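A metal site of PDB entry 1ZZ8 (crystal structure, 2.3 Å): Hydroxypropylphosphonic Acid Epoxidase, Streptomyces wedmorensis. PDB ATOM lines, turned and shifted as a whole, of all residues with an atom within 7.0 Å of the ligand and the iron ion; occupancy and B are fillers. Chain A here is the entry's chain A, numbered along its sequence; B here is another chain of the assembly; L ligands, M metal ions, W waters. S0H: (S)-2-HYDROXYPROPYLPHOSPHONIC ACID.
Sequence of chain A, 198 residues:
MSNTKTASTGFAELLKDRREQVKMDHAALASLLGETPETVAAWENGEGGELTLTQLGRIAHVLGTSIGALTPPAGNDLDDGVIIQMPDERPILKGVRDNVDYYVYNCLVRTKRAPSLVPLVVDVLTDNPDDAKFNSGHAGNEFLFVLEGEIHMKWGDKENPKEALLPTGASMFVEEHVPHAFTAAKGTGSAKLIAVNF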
ATOM      1  N   ARG A  97      -2.269  -5.246   2.329  1.00  0.00           N
ATOM      2  CA  ARG A  97      -1.435  -6.291   1.749  1.00  0.00           C
ATOM      3  C   ARG A  97      -0.102  -5.689   1.370  1.00  0.00           C
ATOM      4  O   ARG A  97      -0.058  -4.701   0.619  1.00  0.00           O
ATOM      5  CB  ARG A  97      -2.074  -6.916   0.510  1.00  0.00           C
ATOM      6  CG  ARG A  97      -3.351  -7.616   0.813  1.00  0.00           C
ATOM      7  CD  ARG A  97      -3.795  -8.539  -0.302  1.00  0.00           C
ATOM      8  NE  ARG A  97      -5.022  -9.191   0.117  1.00  0.00           N
ATOM      9  CZ  ARG A  97      -5.784  -9.951  -0.655  1.00  0.00           C
ATOM     10  NH1 ARG A  97      -5.456 -10.181  -1.927  1.00  0.00           N
ATOM     11  NH2 ARG A  97      -6.891 -10.480  -0.139  1.00  0.00           N
ATOM     12  N   TYR A 102      -5.536  -2.109   0.689  1.00  0.00           N
ATOM     13  CA  TYR A 102      -5.949  -2.740  -0.554  1.00  0.00           C
ATOM     14  C   TYR A 102      -7.464  -2.877  -0.681  1.00  0.00           C
ATOM     15  O   TYR A 102      -8.030  -2.594  -1.725  1.00  0.00           O
ATOM     16  CB  TYR A 102      -5.281  -4.108  -0.645  1.00  0.00           C
ATOM     17  CG  TYR A 102      -5.144  -4.615  -2.049  1.00  0.00           C
ATOM     18  CD1 TYR A 102      -4.167  -4.093  -2.908  1.00  0.00           C
ATOM     19  CD2 TYR A 102      -5.999  -5.599  -2.533  1.00  0.00           C
ATOM     20  CE1 TYR A 102      -4.062  -4.546  -4.215  1.00  0.00           C
ATOM     21  CE2 TYR A 102      -5.898  -6.050  -3.831  1.00  0.00           C
ATOM     22  CZ  TYR A 102      -4.928  -5.533  -4.669  1.00  0.00           C
ATOM     23  OH  TYR A 102      -4.830  -5.992  -5.955  1.00  0.00           O
ATOM     24  N   TYR A 103      -8.110  -3.345   0.391  1.00  0.00           N
ATOM     25  CA  TYR A 103      -9.554  -3.511   0.428  1.00  0.00           C
ATOM     26  C   TYR A 103     -10.031  -3.017   1.775  1.00  0.00           C
ATOM     27  O   TYR A 103      -9.247  -2.836   2.707  1.00  0.00           O
ATOM     28  CB  TYR A 103      -9.986  -4.987   0.369  1.00  0.00           C
ATOM     29  CG  TYR A 103      -9.552  -5.813  -0.801  1.00  0.00           C
ATOM     30  CD1 TYR A 103      -9.658  -5.318  -2.102  1.00  0.00           C
ATOM     31  CD2 TYR A 103      -9.069  -7.117  -0.621  1.00  0.00           C
ATOM     32  CE1 TYR A 103      -9.301  -6.100  -3.194  1.00  0.00           C
ATOM     33  CE2 TYR A 103      -8.719  -7.920  -1.711  1.00  0.00           C
ATOM     34  CZ  TYR A 103      -8.841  -7.391  -2.994  1.00  0.00           C
ATOM     35  OH  TYR A 103      -8.506  -8.148  -4.101  1.00  0.00           O
ATOM     36  N   TYR A 105     -13.302  -4.250   4.160  1.00  0.00           N
ATOM     37  CA  TYR A 105     -14.343  -5.267   4.160  1.00  0.00           C
ATOM     38  C   TYR A 105     -15.576  -4.848   4.948  1.00  0.00           C
ATOM     39  O   TYR A 105     -15.501  -4.670   6.165  1.00  0.00           O
ATOM     40  CB  TYR A 105     -13.836  -6.594   4.740  1.00  0.00           C
ATOM     41  CG  TYR A 105     -12.713  -7.244   3.996  1.00  0.00           C
ATOM     42  CD1 TYR A 105     -11.398  -7.143   4.454  1.00  0.00           C
ATOM     43  CD2 TYR A 105     -12.950  -7.977   2.837  1.00  0.00           C
ATOM     44  CE1 TYR A 105     -10.348  -7.784   3.774  1.00  0.00           C
ATOM     45  CE2 TYR A 105     -11.919  -8.622   2.149  1.00  0.00           C
ATOM     46  CZ  TYR A 105     -10.617  -8.506   2.631  1.00  0.00           C
ATOM     47  OH  TYR A 105      -9.582  -9.101   1.934  1.00  0.00           O
ATOM     48  N   LEU A 120     -20.059 -10.112   1.593  1.00  0.00           N
ATOM     49  CA  LEU A 120     -19.416  -8.835   1.865  1.00  0.00           C
ATOM     50  C   LEU A 120     -19.486  -7.809   0.735  1.00  0.00           C
ATOM     51  O   LEU A 120     -19.641  -8.150  -0.438  1.00  0.00           O
ATOM     52  CB  LEU A 120     -17.918  -9.051   2.119  1.00  0.00           C
ATOM     53  CG  LEU A 120     -17.348 -10.219   2.908  1.00  0.00           C
ATOM     54  CD1 LEU A 120     -15.913 -10.465   2.438  1.00  0.00           C
ATOM     55  CD2 LEU A 120     -17.397  -9.917   4.400  1.00  0.00           C
ATOM     56  N   VAL A 122     -17.052  -5.329  -0.754  1.00  0.00           N
ATOM     57  CA  VAL A 122     -15.617  -5.070  -0.715  1.00  0.00           C
ATOM     58  C   VAL A 122     -15.268  -3.836  -1.533  1.00  0.00           C
ATOM     59  O   VAL A 122     -15.586  -3.774  -2.727  1.00  0.00           O
ATOM     60  CB  VAL A 122     -14.808  -6.261  -1.286  1.00  0.00           C
ATOM     61  CG1 VAL A 122     -13.332  -5.977  -1.177  1.00  0.00           C
ATOM     62  CG2 VAL A 122     -15.179  -7.556  -0.567  1.00  0.00           C
ATOM     63  N   VAL A 124     -12.690  -1.935  -3.515  1.00  0.00           N
ATOM     64  CA  VAL A 124     -11.404  -2.131  -4.158  1.00  0.00           C
ATOM     65  C   VAL A 124     -10.742  -0.747  -4.148  1.00  0.00           C
ATOM     66  O   VAL A 124     -11.097   0.121  -4.939  1.00  0.00           O
ATOM     67  CB  VAL A 124     -11.583  -2.653  -5.596  1.00  0.00           C
ATOM     68  CG1 VAL A 124     -10.223  -2.873  -6.244  1.00  0.00           C
ATOM     69  CG2 VAL A 124     -12.402  -3.943  -5.577  1.00  0.00           C
ATOM     70  N   LYS A 133      -2.321  -6.937  -5.929  1.00  0.00           N
ATOM     71  CA  LYS A 133      -1.799  -7.829  -4.918  1.00  0.00           C
ATOM     72  C   LYS A 133      -2.641  -9.076  -4.659  1.00  0.00           C
ATOM     73  O   LYS A 133      -3.757  -9.018  -4.131  1.00  0.00           O
ATOM     74  CB  LYS A 133      -1.501  -7.055  -3.637  1.00  0.00           C
ATOM     75  CG  LYS A 133      -0.134  -6.390  -3.765  1.00  0.00           C
ATOM     76  CD  LYS A 133       0.121  -5.245  -2.824  1.00  0.00           C
ATOM     77  CE  LYS A 133       1.392  -4.525  -3.281  1.00  0.00           C
ATOM     78  NZ  LYS A 133       1.744  -3.329  -2.463  1.00  0.00           N
ATOM     79  N   PHE A 134      -2.069 -10.200  -5.076  1.00  0.00           N
ATOM     80  CA  PHE A 134      -2.695 -11.511  -4.949  1.00  0.00           C
ATOM     81  C   PHE A 134      -2.832 -12.033  -3.532  1.00  0.00           C
ATOM     82  O   PHE A 134      -2.182 -11.546  -2.607  1.00  0.00           O
ATOM     83  CB  PHE A 134      -1.877 -12.551  -5.730  1.00  0.00           C
ATOM     84  CG  PHE A 134      -2.315 -12.720  -7.143  1.00  0.00           C
ATOM     85  CD1 PHE A 134      -2.181 -11.673  -8.057  1.00  0.00           C
ATOM     86  CD2 PHE A 134      -2.893 -13.905  -7.564  1.00  0.00           C
ATOM     87  CE1 PHE A 134      -2.620 -11.811  -9.354  1.00  0.00           C
ATOM     88  CE2 PHE A 134      -3.345 -14.052  -8.853  1.00  0.00           C
ATOM     89  CZ  PHE A 134      -3.211 -13.005  -9.767  1.00  0.00           C
ATOM     90  N   ASN A 135      -3.726 -12.988  -3.363  1.00  0.00           N
ATOM     91  CA  ASN A 135      -3.853 -13.673  -2.086  1.00  0.00           C
ATOM     92  C   ASN A 135      -3.340 -15.044  -2.543  1.00  0.00           C
ATOM     93  O   ASN A 135      -2.817 -15.156  -3.659  1.00  0.00           O
ATOM     94  CB  ASN A 135      -5.301 -13.730  -1.577  1.00  0.00           C
ATOM     95  CG  ASN A 135      -6.254 -14.401  -2.549  1.00  0.00           C
ATOM     96  OD1 ASN A 135      -5.868 -15.297  -3.308  1.00  0.00           O
ATOM     97  ND2 ASN A 135      -7.514 -13.982  -2.508  1.00  0.00           N
ATOM     98  N   GLY A 137      -5.233 -17.970  -2.708  1.00  0.00           N
ATOM     99  CA  GLY A 137      -6.376 -18.861  -2.773  1.00  0.00           C
ATOM    100  C   GLY A 137      -6.903 -19.049  -1.379  1.00  0.00           C
ATOM    101  O   GLY A 137      -6.199 -18.759  -0.396  1.00  0.00           O
ATOM    102  N   HIS A 138      -8.142 -19.516  -1.267  1.00  0.00           N
ATOM    103  CA  HIS A 138      -8.764 -19.755   0.014  1.00  0.00           C
ATOM    104  C   HIS A 138      -9.848 -20.825  -0.119  1.00  0.00           C
ATOM    105  O   HIS A 138     -10.423 -21.012  -1.199  1.00  0.00           O
ATOM    106  CB  HIS A 138      -9.344 -18.456   0.614  1.00  0.00           C
ATOM    107  CG  HIS A 138     -10.351 -17.772  -0.266  1.00  0.00           C
ATOM    108  ND1 HIS A 138     -11.481 -18.390  -0.747  1.00  0.00           N
ATOM    109  CD2 HIS A 138     -10.414 -16.494  -0.714  1.00  0.00           C
ATOM    110  CE1 HIS A 138     -12.191 -17.530  -1.456  1.00  0.00           C
ATOM    111  NE2 HIS A 138     -11.565 -16.370  -1.448  1.00  0.00           N
ATOM    112  N   GLU A 142     -16.426 -18.691  -4.346  1.00  0.00           N
ATOM    113  CA  GLU A 142     -16.829 -17.307  -4.156  1.00  0.00           C
ATOM    114  C   GLU A 142     -17.563 -16.699  -5.351  1.00  0.00           C
ATOM    115  O   GLU A 142     -17.082 -16.729  -6.493  1.00  0.00           O
ATOM    116  CB  GLU A 142     -15.599 -16.462  -3.801  1.00  0.00           C
ATOM    117  CG  GLU A 142     -15.919 -15.020  -3.471  1.00  0.00           C
ATOM    118  CD  GLU A 142     -14.672 -14.182  -3.152  1.00  0.00           C
ATOM    119  OE1 GLU A 142     -14.806 -12.949  -3.014  1.00  0.00           O
ATOM    120  OE2 GLU A 142     -13.563 -14.764  -3.037  1.00  0.00           O
ATOM    121  N   LEU A 144     -19.069 -13.277  -7.108  1.00  0.00           N
ATOM    122  CA  LEU A 144     -18.802 -11.841  -7.084  1.00  0.00           C
ATOM    123  C   LEU A 144     -19.636 -11.064  -8.082  1.00  0.00           C
ATOM    124  O   LEU A 144     -19.974 -11.558  -9.162  1.00  0.00           O
ATOM    125  CB  LEU A 144     -17.313 -11.556  -7.318  1.00  0.00           C
ATOM    126  CG  LEU A 144     -16.388 -11.989  -6.172  1.00  0.00           C
ATOM    127  CD1 LEU A 144     -15.716 -13.294  -6.568  1.00  0.00           C
ATOM    128  CD2 LEU A 144     -15.347 -10.914  -5.891  1.00  0.00           C
ATOM    129  N   VAL A 174     -15.359 -17.823  -8.639  1.00  0.00           N
ATOM    130  CA  VAL A 174     -13.972 -18.202  -8.402  1.00  0.00           C
ATOM    131  C   VAL A 174     -13.942 -19.465  -7.544  1.00  0.00           C
ATOM    132  O   VAL A 174     -14.255 -19.434  -6.356  1.00  0.00           O
ATOM    133  CB  VAL A 174     -13.196 -17.105  -7.665  1.00  0.00           C
ATOM    134  CG1 VAL A 174     -11.762 -17.548  -7.449  1.00  0.00           C
ATOM    135  CG2 VAL A 174     -13.270 -15.794  -8.442  1.00  0.00           C
ATOM    136  N   VAL A 178      -8.262 -21.248  -5.866  1.00  0.00           N
ATOM    137  CA  VAL A 178      -7.750 -20.438  -6.965  1.00  0.00           C
ATOM    138  C   VAL A 178      -7.357 -19.045  -6.431  1.00  0.00           C
ATOM    139  O   VAL A 178      -8.217 -18.290  -5.945  1.00  0.00           O
ATOM    140  CB  VAL A 178      -8.818 -20.257  -8.056  1.00  0.00           C
ATOM    141  CG1 VAL A 178      -8.286 -19.389  -9.181  1.00  0.00           C
ATOM    142  CG2 VAL A 178      -9.257 -21.630  -8.572  1.00  0.00           C
ATOM    143  N   HIS A 180      -6.418 -15.102  -6.381  1.00  0.00           N
ATOM    144  CA  HIS A 180      -6.937 -14.010  -7.197  1.00  0.00           C
ATOM    145  C   HIS A 180      -6.645 -12.640  -6.593  1.00  0.00           C
ATOM    146  O   HIS A 180      -6.308 -12.534  -5.405  1.00  0.00           O
ATOM    147  CB  HIS A 180      -8.454 -14.191  -7.371  1.00  0.00           C
ATOM    148  CG  HIS A 180      -9.160 -14.536  -6.095  1.00  0.00           C
ATOM    149  ND1 HIS A 180      -9.139 -15.805  -5.556  1.00  0.00           N
ATOM    150  CD2 HIS A 180      -9.860 -13.783  -5.229  1.00  0.00           C
ATOM    151  CE1 HIS A 180      -9.782 -15.811  -4.404  1.00  0.00           C
ATOM    152  NE2 HIS A 180     -10.239 -14.591  -4.180  1.00  0.00           N
ATOM    153  N   ALA A 181      -6.815 -11.612  -7.410  1.00  0.00           N
ATOM    154  CA  ALA A 181      -6.581 -10.234  -7.015  1.00  0.00           C
ATOM    155  C   ALA A 181      -7.451  -9.273  -7.823  1.00  0.00           C
ATOM    156  O   ALA A 181      -7.775  -9.537  -8.981  1.00  0.00           O
ATOM    157  CB  ALA A 181      -5.119  -9.892  -7.219  1.00  0.00           C
ATOM    158  N   PHE A 182      -7.840  -8.156  -7.205  1.00  0.00           N
ATOM    159  CA  PHE A 182      -8.666  -7.153  -7.877  1.00  0.00           C
ATOM    160  C   PHE A 182      -8.142  -5.742  -7.634  1.00  0.00           C
ATOM    161  O   PHE A 182      -7.522  -5.450  -6.612  1.00  0.00           O
ATOM    162  CB  PHE A 182     -10.130  -7.204  -7.411  1.00  0.00           C
ATOM    163  CG  PHE A 182     -10.814  -8.528  -7.613  1.00  0.00           C
ATOM    164  CD1 PHE A 182     -10.766  -9.507  -6.640  1.00  0.00           C
ATOM    165  CD2 PHE A 182     -11.513  -8.786  -8.782  1.00  0.00           C
ATOM    166  CE1 PHE A 182     -11.409 -10.725  -6.813  1.00  0.00           C
ATOM    167  CE2 PHE A 182     -12.158 -10.000  -8.979  1.00  0.00           C
ATOM    168  CZ  PHE A 182     -12.110 -10.972  -7.984  1.00  0.00           C
ATOM    169  N   LEU A 193     -17.431  -4.155  -5.001  1.00  0.00           N
ATOM    170  CA  LEU A 193     -18.016  -5.428  -5.360  1.00  0.00           C
ATOM    171  C   LEU A 193     -18.630  -6.168  -4.190  1.00  0.00           C
ATOM    172  O   LEU A 193     -18.246  -5.962  -3.036  1.00  0.00           O
ATOM    173  CB  LEU A 193     -16.960  -6.321  -6.048  1.00  0.00           C
ATOM    174  CG  LEU A 193     -15.643  -6.632  -5.341  1.00  0.00           C
ATOM    175  CD1 LEU A 193     -15.921  -7.380  -4.043  1.00  0.00           C
ATOM    176  CD2 LEU A 193     -14.742  -7.485  -6.237  1.00  0.00           C
ATOM    177  N   ALA A 195     -19.008  -9.683  -2.474  1.00  0.00           N
ATOM    178  CA  ALA A 195     -18.361 -10.983  -2.500  1.00  0.00           C
ATOM    179  C   ALA A 195     -19.059 -11.951  -1.556  1.00  0.00           C
ATOM    180  O   ALA A 195     -19.187 -11.687  -0.354  1.00  0.00           O
ATOM    181  CB  ALA A 195     -16.897 -10.821  -2.109  1.00  0.00           C
ATOM    182  N   ASN A 197     -18.848 -15.698  -0.130  1.00  0.00           N
ATOM    183  CA  ASN A 197     -18.101 -16.941   0.048  1.00  0.00           C
ATOM    184  C   ASN A 197     -19.121 -17.896   0.643  1.00  0.00           C
ATOM    185  O   ASN A 197     -19.817 -17.538   1.588  1.00  0.00           O
ATOM    186  CB  ASN A 197     -16.934 -16.748   1.014  1.00  0.00           C
ATOM    187  CG  ASN A 197     -15.970 -15.657   0.554  1.00  0.00           C
ATOM    188  OD1 ASN A 197     -15.217 -15.838  -0.414  1.00  0.00           O
ATOM    189  ND2 ASN A 197     -15.994 -14.511   1.238  1.00  0.00           N
ATOM    190  N   GLU B  20      -9.688 -15.445   9.736  1.00  0.00           N
ATOM    191  CA  GLU B  20      -9.425 -14.808   8.455  1.00  0.00           C
ATOM    192  C   GLU B  20     -10.565 -14.937   7.443  1.00  0.00           C
ATOM    193  O   GLU B  20     -10.763 -14.042   6.609  1.00  0.00           O
ATOM    194  CB  GLU B  20      -8.129 -15.358   7.850  1.00  0.00           C
ATOM    195  CG  GLU B  20      -6.864 -14.946   8.622  1.00  0.00           C
ATOM    196  CD  GLU B  20      -5.568 -15.424   7.978  1.00  0.00           C
ATOM    197  OE1 GLU B  20      -4.502 -14.839   8.289  1.00  0.00           O
ATOM    198  OE2 GLU B  20      -5.614 -16.382   7.174  1.00  0.00           O
ATOM    199  N   LYS B  23     -13.175 -12.191   8.236  1.00  0.00           N
ATOM    200  CA  LYS B  23     -12.671 -10.830   8.266  1.00  0.00           C
ATOM    201  C   LYS B  23     -12.584 -10.152   9.625  1.00  0.00           C
ATOM    202  O   LYS B  23     -13.240  -9.135   9.879  1.00  0.00           O
ATOM    203  CB  LYS B  23     -13.493  -9.964   7.321  1.00  0.00           C
ATOM    204  CG  LYS B  23     -13.026 -10.058   5.881  1.00  0.00           C
ATOM    205  CD  LYS B  23     -12.965 -11.492   5.425  1.00  0.00           C
ATOM    206  CE  LYS B  23     -12.229 -11.585   4.136  1.00  0.00           C
ATOM    207  NZ  LYS B  23     -12.067 -13.000   3.746  1.00  0.00           N
HETATM  208  P1  S0H L   1     -10.154 -11.792  -0.579  1.00  0.00           P
HETATM  209  C2  S0H L   1     -11.524 -10.734  -1.127  1.00  0.00           C
HETATM  210  C3  S0H L   1     -11.597 -10.735  -2.653  1.00  0.00           C
HETATM  211  O6  S0H L   1     -12.401 -11.793  -3.084  1.00  0.00           O
HETATM  212  C1  S0H L   1     -12.091  -9.811  -2.991  1.00  0.00           C
HETATM  213  O13 S0H L   1      -8.915 -11.564  -1.293  1.00  0.00           O
HETATM  214  O14 S0H L   1     -10.620 -13.280  -0.709  1.00  0.00           O
HETATM  215  O15 S0H L   1     -10.021 -11.704   0.967  1.00  0.00           O
HETATM  216 FE    FE M   1     -11.649 -14.147  -2.284  1.00  0.00          FE
HETATM  217  O   HOH W   1      -7.804 -10.715  -3.561  1.00  0.00           O
HETATM  218  O   HOH W   2     -13.744 -13.067  -0.483  1.00  0.00           O
HETATM  219  O   HOH W   3     -11.572 -14.221   1.575  1.00  0.00           O
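The side-chain amino group (NZ) of Lys 23 of chain B is in salt-bridge range of an oxygen (O15) of the ligand. O13 of the ligand is in salt-bridge range of NH2 of Arg 97 (2.6 Å). OH of Tyr 105 sits at hydrogen-bond distance from O15 of the ligand, at 2.8 Å. The side-chain amide nitrogen of Asn 135 lies within hydrogen-bond range of an oxygen (O13) of the ligand (3.0 Å).
OD1 of Asn 197 lies close to OE2 of Glu 142, 3.3 Å away. The backbone carbonyl oxygen (O) of Phe 182 is in hydrogen-bond range of the side-chain hydroxyl (OH) of Tyr 102, at 2.8 Å. The side-chain amide oxygen of Asn 135 lies within hydrogen-bond range of the backbone NH of His 180. A ring nitrogen (ND1) of His 180 sits at hydrogen-bond distance from the backbone carbonyl oxygen (O) of Val 178 (2.7 Å). The backbone carbonyl oxygen (O) of Glu 142 is in hydrogen-bond range of the backbone NH (N) of Val 174 (3.0 Å). The backbone carbonyl oxygen (O) of Lys 133 lies within hydrogen-bond range of the guanidinium group (NH1) of Arg 97 (3.0 Å). NZ of Lys 23 of chain B is in hydrogen-bond range of O of Glu 20 of chain B. The side-chain hydroxyl (OH) of Tyr 103 lies within hydrogen-bond range of the backbone NH (N) of Phe 182 (3.2 Å).
Tyr 103 touches the ligand (CE2 to O13, 3.7 Å). CD1 of Phe 182 touches C1 of the ligand (3.9 Å). Along chain A the residues within 4 Å of the ligand span positions 97 to 182.
Of the 24 residues printed, 3 come within 4 Å of the iron ion.
The iron ion is bound by O14 of the ligand (2.1 Å), OE2 of Glu 142 (2.1 Å), NE2 of His 138 (2.4 Å), NE2 of His 180 (2.4 Å) and O6 of the ligand (2.6 Å). The iron ion has five donor atoms within binding distance.
Water W3 lies within hydrogen-bond range of NZ of Lys 23 of chain B (2.5 Å) and O15 of the ligand (3.0 Å). Water W1 lies within hydrogen-bond range of O13 of the ligand (2.7 Å), OH of Tyr 103 (2.7 Å), NH1 of Arg 97 (2.9 Å), O of His 180 (3.0 Å) and ND2 of Asn 135 (3.4 Å). Water W2 bridges OE1 of Glu 142 (2.7 Å) and OD1 of Asn 197 (3.1 Å).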
